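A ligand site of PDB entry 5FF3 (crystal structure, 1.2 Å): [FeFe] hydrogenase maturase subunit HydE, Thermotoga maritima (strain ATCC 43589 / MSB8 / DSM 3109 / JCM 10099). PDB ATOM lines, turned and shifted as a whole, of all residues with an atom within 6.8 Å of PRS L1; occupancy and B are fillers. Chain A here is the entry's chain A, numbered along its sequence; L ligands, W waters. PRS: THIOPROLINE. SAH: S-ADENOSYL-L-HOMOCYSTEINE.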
ATOM      1  N   ILE A  56     -16.525   5.665  30.944  1.00  0.00           N
ATOM      2  CA  ILE A  56     -15.215   5.102  31.046  1.00  0.00           C
ATOM      3  C   ILE A  56     -14.951   4.500  32.402  1.00  0.00           C
ATOM      4  O   ILE A  56     -15.161   5.141  33.422  1.00  0.00           O
ATOM      5  CB  ILE A  56     -14.106   6.127  30.630  1.00  0.00           C
ATOM      6  CG1 ILE A  56     -12.727   5.435  30.549  1.00  0.00           C
ATOM      7  CG2 ILE A  56     -14.082   7.356  31.470  1.00  0.00           C
ATOM      8  CD1 ILE A  56     -11.699   6.258  29.819  1.00  0.00           C
ATOM      9  N   GLU A  58     -11.857   2.923  34.397  1.00  0.00           N
ATOM     10  CA  GLU A  58     -10.387   2.833  34.443  1.00  0.00           C
ATOM     11  C   GLU A  58     -10.106   1.720  35.422  1.00  0.00           C
ATOM     12  O   GLU A  58     -10.119   1.904  36.655  1.00  0.00           O
ATOM     13  CB  GLU A  58      -9.802   4.171  34.885  1.00  0.00           C
ATOM     14  CG  GLU A  58     -10.200   5.360  34.000  1.00  0.00           C
ATOM     15  CD  GLU A  58     -10.318   6.715  34.704  1.00  0.00           C
ATOM     16  OE1 GLU A  58     -10.675   6.727  35.903  1.00  0.00           O
ATOM     17  OE2 GLU A  58     -10.133   7.747  34.032  1.00  0.00           O
ATOM     18  N   GLN A 107     -10.501   1.210  30.096  1.00  0.00           N
ATOM     19  CA  GLN A 107      -9.153   1.791  29.976  1.00  0.00           C
ATOM     20  C   GLN A 107      -8.322   1.339  31.168  1.00  0.00           C
ATOM     21  O   GLN A 107      -8.812   1.189  32.292  1.00  0.00           O
ATOM     22  CB  GLN A 107      -9.177   3.338  29.900  1.00  0.00           C
ATOM     23  CG  GLN A 107      -7.792   3.910  29.570  1.00  0.00           C
ATOM     24  CD  GLN A 107      -7.843   5.394  29.444  1.00  0.00           C
ATOM     25  OE1 GLN A 107      -7.776   6.118  30.465  1.00  0.00           O
ATOM     26  NE2 GLN A 107      -7.888   5.914  28.246  1.00  0.00           N
ATOM     27  N   SER A 136      -9.178   0.654  25.569  1.00  0.00           N
ATOM     28  CA  SER A 136      -8.050   1.563  25.548  1.00  0.00           C
ATOM     29  C   SER A 136      -7.001   1.016  26.508  1.00  0.00           C
ATOM     30  O   SER A 136      -6.859   1.436  27.637  1.00  0.00           O
ATOM     31  CB  SER A 136      -8.532   2.947  25.968  1.00  0.00           C
ATOM     32  OG  SER A 136      -7.489   3.932  25.938  1.00  0.00           O
ATOM     33  N   LEU A 157      -9.099   2.853  21.333  1.00  0.00           N
ATOM     34  CA  LEU A 157      -8.436   4.134  21.429  1.00  0.00           C
ATOM     35  C   LEU A 157      -6.957   3.971  21.689  1.00  0.00           C
ATOM     36  O   LEU A 157      -6.580   3.303  22.661  1.00  0.00           O
ATOM     37  CB  LEU A 157      -9.031   4.959  22.587  1.00  0.00           C
ATOM     38  CG  LEU A 157     -10.532   5.102  22.646  1.00  0.00           C
ATOM     39  CD1 LEU A 157     -10.928   5.854  23.886  1.00  0.00           C
ATOM     40  CD2 LEU A 157     -11.099   5.715  21.364  1.00  0.00           C
ATOM     41  N   ARG A 159      -4.081   6.729  21.318  1.00  0.00           N
ATOM     42  CA  ARG A 159      -3.579   7.992  20.864  1.00  0.00           C
ATOM     43  C   ARG A 159      -2.153   7.861  20.310  1.00  0.00           C
ATOM     44  O   ARG A 159      -1.335   7.147  20.871  1.00  0.00           O
ATOM     45  CB  ARG A 159      -3.528   8.981  21.969  1.00  0.00           C
ATOM     46  CG  ARG A 159      -4.904   9.406  22.421  1.00  0.00           C
ATOM     47  CD  ARG A 159      -4.732  10.476  23.459  1.00  0.00           C
ATOM     48  NE  ARG A 159      -5.988  10.918  24.003  1.00  0.00           N
ATOM     49  CZ  ARG A 159      -6.118  11.975  24.788  1.00  0.00           C
ATOM     50  NH1 ARG A 159      -5.013  12.568  25.213  1.00  0.00           N
ATOM     51  NH2 ARG A 159      -7.312  12.403  25.176  1.00  0.00           N
ATOM     52  N   GLY A 226      -8.710  11.923  20.012  1.00  0.00           N
ATOM     53  CA  GLY A 226      -8.648  12.406  21.400  1.00  0.00           C
ATOM     54  C   GLY A 226      -7.487  13.338  21.580  1.00  0.00           C
ATOM     55  O   GLY A 226      -6.335  12.932  21.401  1.00  0.00           O
ATOM     56  N   ILE A 227      -7.832  14.602  21.919  1.00  0.00           N
ATOM     57  CA  ILE A 227      -6.809  15.619  22.115  1.00  0.00           C
ATOM     58  C   ILE A 227      -6.968  16.262  23.448  1.00  0.00           C
ATOM     59  O   ILE A 227      -8.102  16.580  23.873  1.00  0.00           O
ATOM     60  CB  ILE A 227      -6.952  16.692  20.986  1.00  0.00           C
ATOM     61  CG1 ILE A 227      -6.583  16.064  19.598  1.00  0.00           C
ATOM     62  CG2 ILE A 227      -6.115  17.938  21.246  1.00  0.00           C
ATOM     63  CD1 ILE A 227      -6.955  16.857  18.376  1.00  0.00           C
ATOM     64  N   GLY A 228      -5.848  16.484  24.144  1.00  0.00           N
ATOM     65  CA  GLY A 228      -5.893  17.282  25.325  1.00  0.00           C
ATOM     66  C   GLY A 228      -4.521  17.866  25.538  1.00  0.00           C
ATOM     67  O   GLY A 228      -3.555  17.513  24.921  1.00  0.00           O
ATOM     68  N   PRO A 229      -4.473  18.724  26.542  1.00  0.00           N
ATOM     69  CA  PRO A 229      -3.200  19.306  26.930  1.00  0.00           C
ATOM     70  C   PRO A 229      -2.430  18.322  27.722  1.00  0.00           C
ATOM     71  O   PRO A 229      -2.920  17.456  28.403  1.00  0.00           O
ATOM     72  CB  PRO A 229      -3.610  20.449  27.874  1.00  0.00           C
ATOM     73  CG  PRO A 229      -4.844  19.919  28.560  1.00  0.00           C
ATOM     74  CD  PRO A 229      -5.550  19.201  27.435  1.00  0.00           C
ATOM     75  N   PRO A 266     -13.884  13.734  21.273  1.00  0.00           N
ATOM     76  CA  PRO A 266     -14.291  14.038  22.645  1.00  0.00           C
ATOM     77  C   PRO A 266     -13.823  15.414  23.090  1.00  0.00           C
ATOM     78  O   PRO A 266     -12.825  15.965  22.680  1.00  0.00           O
ATOM     79  CB  PRO A 266     -13.575  12.956  23.453  1.00  0.00           C
ATOM     80  CG  PRO A 266     -13.301  11.823  22.519  1.00  0.00           C
ATOM     81  CD  PRO A 266     -13.013  12.555  21.212  1.00  0.00           C
ATOM     82  N   ALA A 267     -14.581  15.934  24.064  1.00  0.00           N
ATOM     83  CA  ALA A 267     -14.179  17.014  24.938  1.00  0.00           C
ATOM     84  C   ALA A 267     -13.552  16.331  26.135  1.00  0.00           C
ATOM     85  O   ALA A 267     -14.284  15.821  26.987  1.00  0.00           O
ATOM     86  CB  ALA A 267     -15.381  17.890  25.317  1.00  0.00           C
ATOM     87  N   THR A 268     -12.245  16.275  26.211  1.00  0.00           N
ATOM     88  CA  THR A 268     -11.579  15.431  27.187  1.00  0.00           C
ATOM     89  C   THR A 268     -11.590  15.986  28.601  1.00  0.00           C
ATOM     90  O   THR A 268     -11.649  17.184  28.848  1.00  0.00           O
ATOM     91  CB  THR A 268     -10.169  15.161  26.735  1.00  0.00           C
ATOM     92  OG1 THR A 268      -9.427  16.376  26.684  1.00  0.00           O
ATOM     93  CG2 THR A 268     -10.105  14.400  25.422  1.00  0.00           C
ATOM     94  N   THR A 269     -11.470  15.065  29.561  1.00  0.00           N
ATOM     95  CA  THR A 269     -11.359  15.457  30.940  1.00  0.00           C
ATOM     96  C   THR A 269     -10.160  16.362  31.197  1.00  0.00           C
ATOM     97  O   THR A 269     -10.253  17.268  31.999  1.00  0.00           O
ATOM     98  CB  THR A 269     -11.364  14.235  31.871  1.00  0.00           C
ATOM     99  OG1 THR A 269     -12.639  13.609  31.717  1.00  0.00           O
ATOM    100  CG2 THR A 269     -11.176  14.593  33.344  1.00  0.00           C
ATOM    101  N   ALA A 270      -9.069  16.150  30.460  1.00  0.00           N
ATOM    102  CA  ALA A 270      -7.898  17.033  30.643  1.00  0.00           C
ATOM    103  C   ALA A 270      -8.268  18.462  30.274  1.00  0.00           C
ATOM    104  O   ALA A 270      -7.798  19.400  30.937  1.00  0.00           O
ATOM    105  CB  ALA A 270      -6.720  16.522  29.848  1.00  0.00           C
ATOM    106  N   MET A 271      -9.086  18.684  29.261  1.00  0.00           N
ATOM    107  CA  MET A 271      -9.552  20.052  28.940  1.00  0.00           C
ATOM    108  C   MET A 271     -10.351  20.649  30.090  1.00  0.00           C
ATOM    109  O   MET A 271     -10.217  21.832  30.356  1.00  0.00           O
ATOM    110  CB  MET A 271     -10.379  20.036  27.652  1.00  0.00           C
ATOM    111  CG  MET A 271      -9.475  19.861  26.388  1.00  0.00           C
ATOM    112  SD  MET A 271      -8.371  21.208  26.105  1.00  0.00           S
ATOM    113  CE  MET A 271      -9.224  22.119  24.781  1.00  0.00           C
ATOM    114  N   THR A 273      -9.929  19.874  33.219  1.00  0.00           N
ATOM    115  CA  THR A 273      -9.000  19.991  34.328  1.00  0.00           C
ATOM    116  C   THR A 273      -8.194  21.273  34.280  1.00  0.00           C
ATOM    117  O   THR A 273      -7.995  21.909  35.331  1.00  0.00           O
ATOM    118  CB  THR A 273      -8.131  18.704  34.395  1.00  0.00           C
ATOM    119  OG1 THR A 273      -8.976  17.574  34.563  1.00  0.00           O
ATOM    120  CG2 THR A 273      -7.164  18.741  35.577  1.00  0.00           C
ATOM    121  N   MET A 291     -16.838  11.718  27.824  1.00  0.00           N
ATOM    122  CA  MET A 291     -16.541  10.441  28.476  1.00  0.00           C
ATOM    123  C   MET A 291     -16.647  10.617  30.064  1.00  0.00           C
ATOM    124  O   MET A 291     -15.660  10.837  30.736  1.00  0.00           O
ATOM    125  CB  MET A 291     -15.190   9.923  28.099  1.00  0.00           C
ATOM    126  CG  MET A 291     -15.062   9.661  26.583  1.00  0.00           C
ATOM    127  SD  MET A 291     -13.763   8.410  26.336  1.00  0.00           S
ATOM    128  CE  MET A 291     -13.744   8.508  24.577  1.00  0.00           C
ATOM    129  N   TYR A 303      -6.364   6.696  39.847  1.00  0.00           N
ATOM    130  CA  TYR A 303      -6.091   6.655  38.418  1.00  0.00           C
ATOM    131  C   TYR A 303      -5.703   8.001  37.961  1.00  0.00           C
ATOM    132  O   TYR A 303      -6.549   8.795  37.523  1.00  0.00           O
ATOM    133  CB  TYR A 303      -7.268   6.091  37.641  1.00  0.00           C
ATOM    134  CG  TYR A 303      -6.917   5.741  36.198  1.00  0.00           C
ATOM    135  CD1 TYR A 303      -6.379   4.461  35.878  1.00  0.00           C
ATOM    136  CD2 TYR A 303      -7.098   6.647  35.178  1.00  0.00           C
ATOM    137  CE1 TYR A 303      -6.086   4.112  34.592  1.00  0.00           C
ATOM    138  CE2 TYR A 303      -6.831   6.305  33.898  1.00  0.00           C
ATOM    139  CZ  TYR A 303      -6.287   5.060  33.598  1.00  0.00           C
ATOM    140  OH  TYR A 303      -6.044   4.678  32.260  1.00  0.00           O
ATOM    141  N   LEU A 305      -3.286   9.789  35.704  1.00  0.00           N
ATOM    142  CA  LEU A 305      -2.376  10.049  34.590  1.00  0.00           C
ATOM    143  C   LEU A 305      -1.755  11.378  34.821  1.00  0.00           C
ATOM    144  O   LEU A 305      -0.547  11.582  34.579  1.00  0.00           O
ATOM    145  CB  LEU A 305      -3.192  10.039  33.273  1.00  0.00           C
ATOM    146  CG  LEU A 305      -3.988   8.747  32.977  1.00  0.00           C
ATOM    147  CD1 LEU A 305      -4.912   9.018  31.789  1.00  0.00           C
ATOM    148  CD2 LEU A 305      -3.041   7.588  32.710  1.00  0.00           C
ATOM    149  N   TYR A 306      -2.546  12.353  35.253  1.00  0.00           N
ATOM    150  CA  TYR A 306      -2.165  13.686  35.616  1.00  0.00           C
ATOM    151  C   TYR A 306      -2.904  14.041  36.868  1.00  0.00           C
ATOM    152  O   TYR A 306      -3.901  13.398  37.222  1.00  0.00           O
ATOM    153  CB  TYR A 306      -2.417  14.737  34.529  1.00  0.00           C
ATOM    154  CG  TYR A 306      -3.830  14.676  33.975  1.00  0.00           C
ATOM    155  CD1 TYR A 306      -4.888  15.341  34.647  1.00  0.00           C
ATOM    156  CD2 TYR A 306      -4.148  13.921  32.901  1.00  0.00           C
ATOM    157  CE1 TYR A 306      -6.155  15.277  34.190  1.00  0.00           C
ATOM    158  CE2 TYR A 306      -5.458  13.802  32.421  1.00  0.00           C
ATOM    159  CZ  TYR A 306      -6.452  14.533  33.095  1.00  0.00           C
ATOM    160  OH  TYR A 306      -7.770  14.455  32.699  1.00  0.00           O
ATOM    161  N   LYS A 309      -7.278  16.040  38.657  1.00  0.00           N
ATOM    162  CA  LYS A 309      -8.342  15.699  37.692  1.00  0.00           C
ATOM    163  C   LYS A 309      -9.699  16.002  38.324  1.00  0.00           C
ATOM    164  O   LYS A 309      -9.964  15.702  39.506  1.00  0.00           O
ATOM    165  CB  LYS A 309      -8.225  14.202  37.352  1.00  0.00           C
ATOM    166  CG  LYS A 309      -9.097  13.600  36.211  1.00  0.00           C
ATOM    167  CD  LYS A 309      -8.931  12.024  36.329  1.00  0.00           C
ATOM    168  CE  LYS A 309      -9.670  11.028  35.446  1.00  0.00           C
ATOM    169  NZ  LYS A 309      -8.864   9.815  35.584  1.00  0.00           N
HETATM  170  N   PRS L   1      -9.308  11.187  28.120  1.00  0.00           N
HETATM  171  CD  PRS L   1      -9.171   9.831  27.467  1.00  0.00           C
HETATM  172  CA  PRS L   1      -8.572  11.166  29.412  1.00  0.00           C
HETATM  173  CB  PRS L   1      -7.293  10.478  29.018  1.00  0.00           C
HETATM  174  SG  PRS L   1      -7.454   9.361  27.508  1.00  0.00           S
HETATM  175  C   PRS L   1      -8.404  12.523  30.018  1.00  0.00           C
HETATM  176  O   PRS L   1      -8.454  13.513  29.379  1.00  0.00           O
HETATM  177  OXT PRS L   1      -8.261  12.437  31.273  1.00  0.00           O
HETATM  178  N   SAH L   2      -2.038   2.994  28.688  1.00  0.00           N
HETATM  179  CA  SAH L   2      -2.966   3.328  27.614  1.00  0.00           C
HETATM  180  CB  SAH L   2      -4.263   3.987  28.181  1.00  0.00           C
HETATM  181  CG  SAH L   2      -4.174   4.991  29.302  1.00  0.00           C
HETATM  182  SD  SAH L   2      -3.146   6.399  29.080  1.00  0.00           S
HETATM  183  C   SAH L   2      -2.261   4.128  26.614  1.00  0.00           C
HETATM  184  O   SAH L   2      -2.786   4.223  25.486  1.00  0.00           O
HETATM  185  OXT SAH L   2      -1.135   4.610  26.921  1.00  0.00           O
HETATM  186  C5' SAH L   2      -4.400   7.400  28.126  1.00  0.00           C
HETATM  187  C4' SAH L   2      -3.932   8.768  27.555  1.00  0.00           C
HETATM  188  O4' SAH L   2      -3.733   9.754  28.620  1.00  0.00           O
HETATM  189  C3' SAH L   2      -2.672   8.798  26.850  1.00  0.00           C
HETATM  190  O3' SAH L   2      -2.880   8.350  25.505  1.00  0.00           O
HETATM  191  C2' SAH L   2      -2.107  10.231  26.958  1.00  0.00           C
HETATM  192  O2' SAH L   2      -2.403  11.048  25.820  1.00  0.00           O
HETATM  193  C1' SAH L   2      -2.866  10.816  28.137  1.00  0.00           C
HETATM  194  N9  SAH L   2      -2.091  11.233  29.266  1.00  0.00           N
HETATM  195  C8  SAH L   2      -1.166  10.504  29.931  1.00  0.00           C
HETATM  196  N7  SAH L   2      -0.471  11.211  30.797  1.00  0.00           N
HETATM  197  C5  SAH L   2      -0.917  12.494  30.647  1.00  0.00           C
HETATM  198  C6  SAH L   2      -0.586  13.745  31.242  1.00  0.00           C
HETATM  199  N6  SAH L   2       0.418  13.906  32.110  1.00  0.00           N
HETATM  200  N1  SAH L   2      -1.255  14.849  30.823  1.00  0.00           N
HETATM  201  C2  SAH L   2      -2.267  14.769  29.918  1.00  0.00           C
HETATM  202  N3  SAH L   2      -2.630  13.650  29.358  1.00  0.00           N
HETATM  203  C4  SAH L   2      -1.982  12.521  29.672  1.00  0.00           C
HETATM  204  O   HOH W   1      -7.012  14.345  27.193  1.00  0.00           O
HETATM  205  O   HOH W   2      -7.948  10.419  32.984  1.00  0.00           O
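The side-chain amide nitrogen (NE2) of Gln 107 sits close to a sulfur (SG) of PRS L1 (3.6 Å).
O of PRS L1 sits at hydrogen-bond distance from N of Ala 270 (2.9 Å).
The backbone NH of Thr 269 lies within hydrogen-bond range of an oxygen (O) of PRS L1 (3.4 Å).
The guanidinium group (NH1) of Arg 159 is in hydrogen-bond range of an oxygen (O2') of SAH L2, 3.1 Å away.
The side-chain hydroxyl (OH) of Tyr 306 is in hydrogen-bond range of an oxygen (OXT) of PRS L1 (2.5 Å).
The side-chain hydroxyl (OH) of Tyr 306 is in hydrogen-bond range of the backbone NH (N) of Ala 270 (3.1 Å).
The backbone carbonyl oxygen of Gly 226 sits at hydrogen-bond distance from the guanidinium group of Arg 159.
O of Thr 269 is in hydrogen-bond range of OG1 of Thr 273 (2.9 Å).
OG of Ser 136 lies within hydrogen-bond range of NE2 of Gln 107 (3.1 Å).
OG1 of Thr 268 sits at hydrogen-bond distance from O of Ile 227 (3.1 Å).
N of Met 271 is in hydrogen-bond range of OG1 of Thr 268 (3.5 Å).
The side-chain amide oxygen (OE1) of Gln 107 lies within hydrogen-bond range of the side-chain hydroxyl (OH) of Tyr 303, 2.9 Å away.
NH2 of Arg 159 touches N of PRS L1 (3.8 Å).
Thr 268 touches PRS L1.
Leu 305 touches PRS L1 (CD1 to CB, 3.9 Å).
Hydrophobic or aromatic side chains that line PRS L1: Ala 270, Leu 305 and Tyr 306.
Of the 22 residues printed, 7 come within 4 Å of PRS L1.
Along chain A the residues within 4 Å of PRS L1 span positions 107 to 306.
Water W2 lies within hydrogen-bond range of OXT of PRS L1 and NZ of Lys 309.
Water W1 lies within hydrogen-bond range of O of PRS L1, NH2 of Arg 159 and OG1 of Thr 268.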
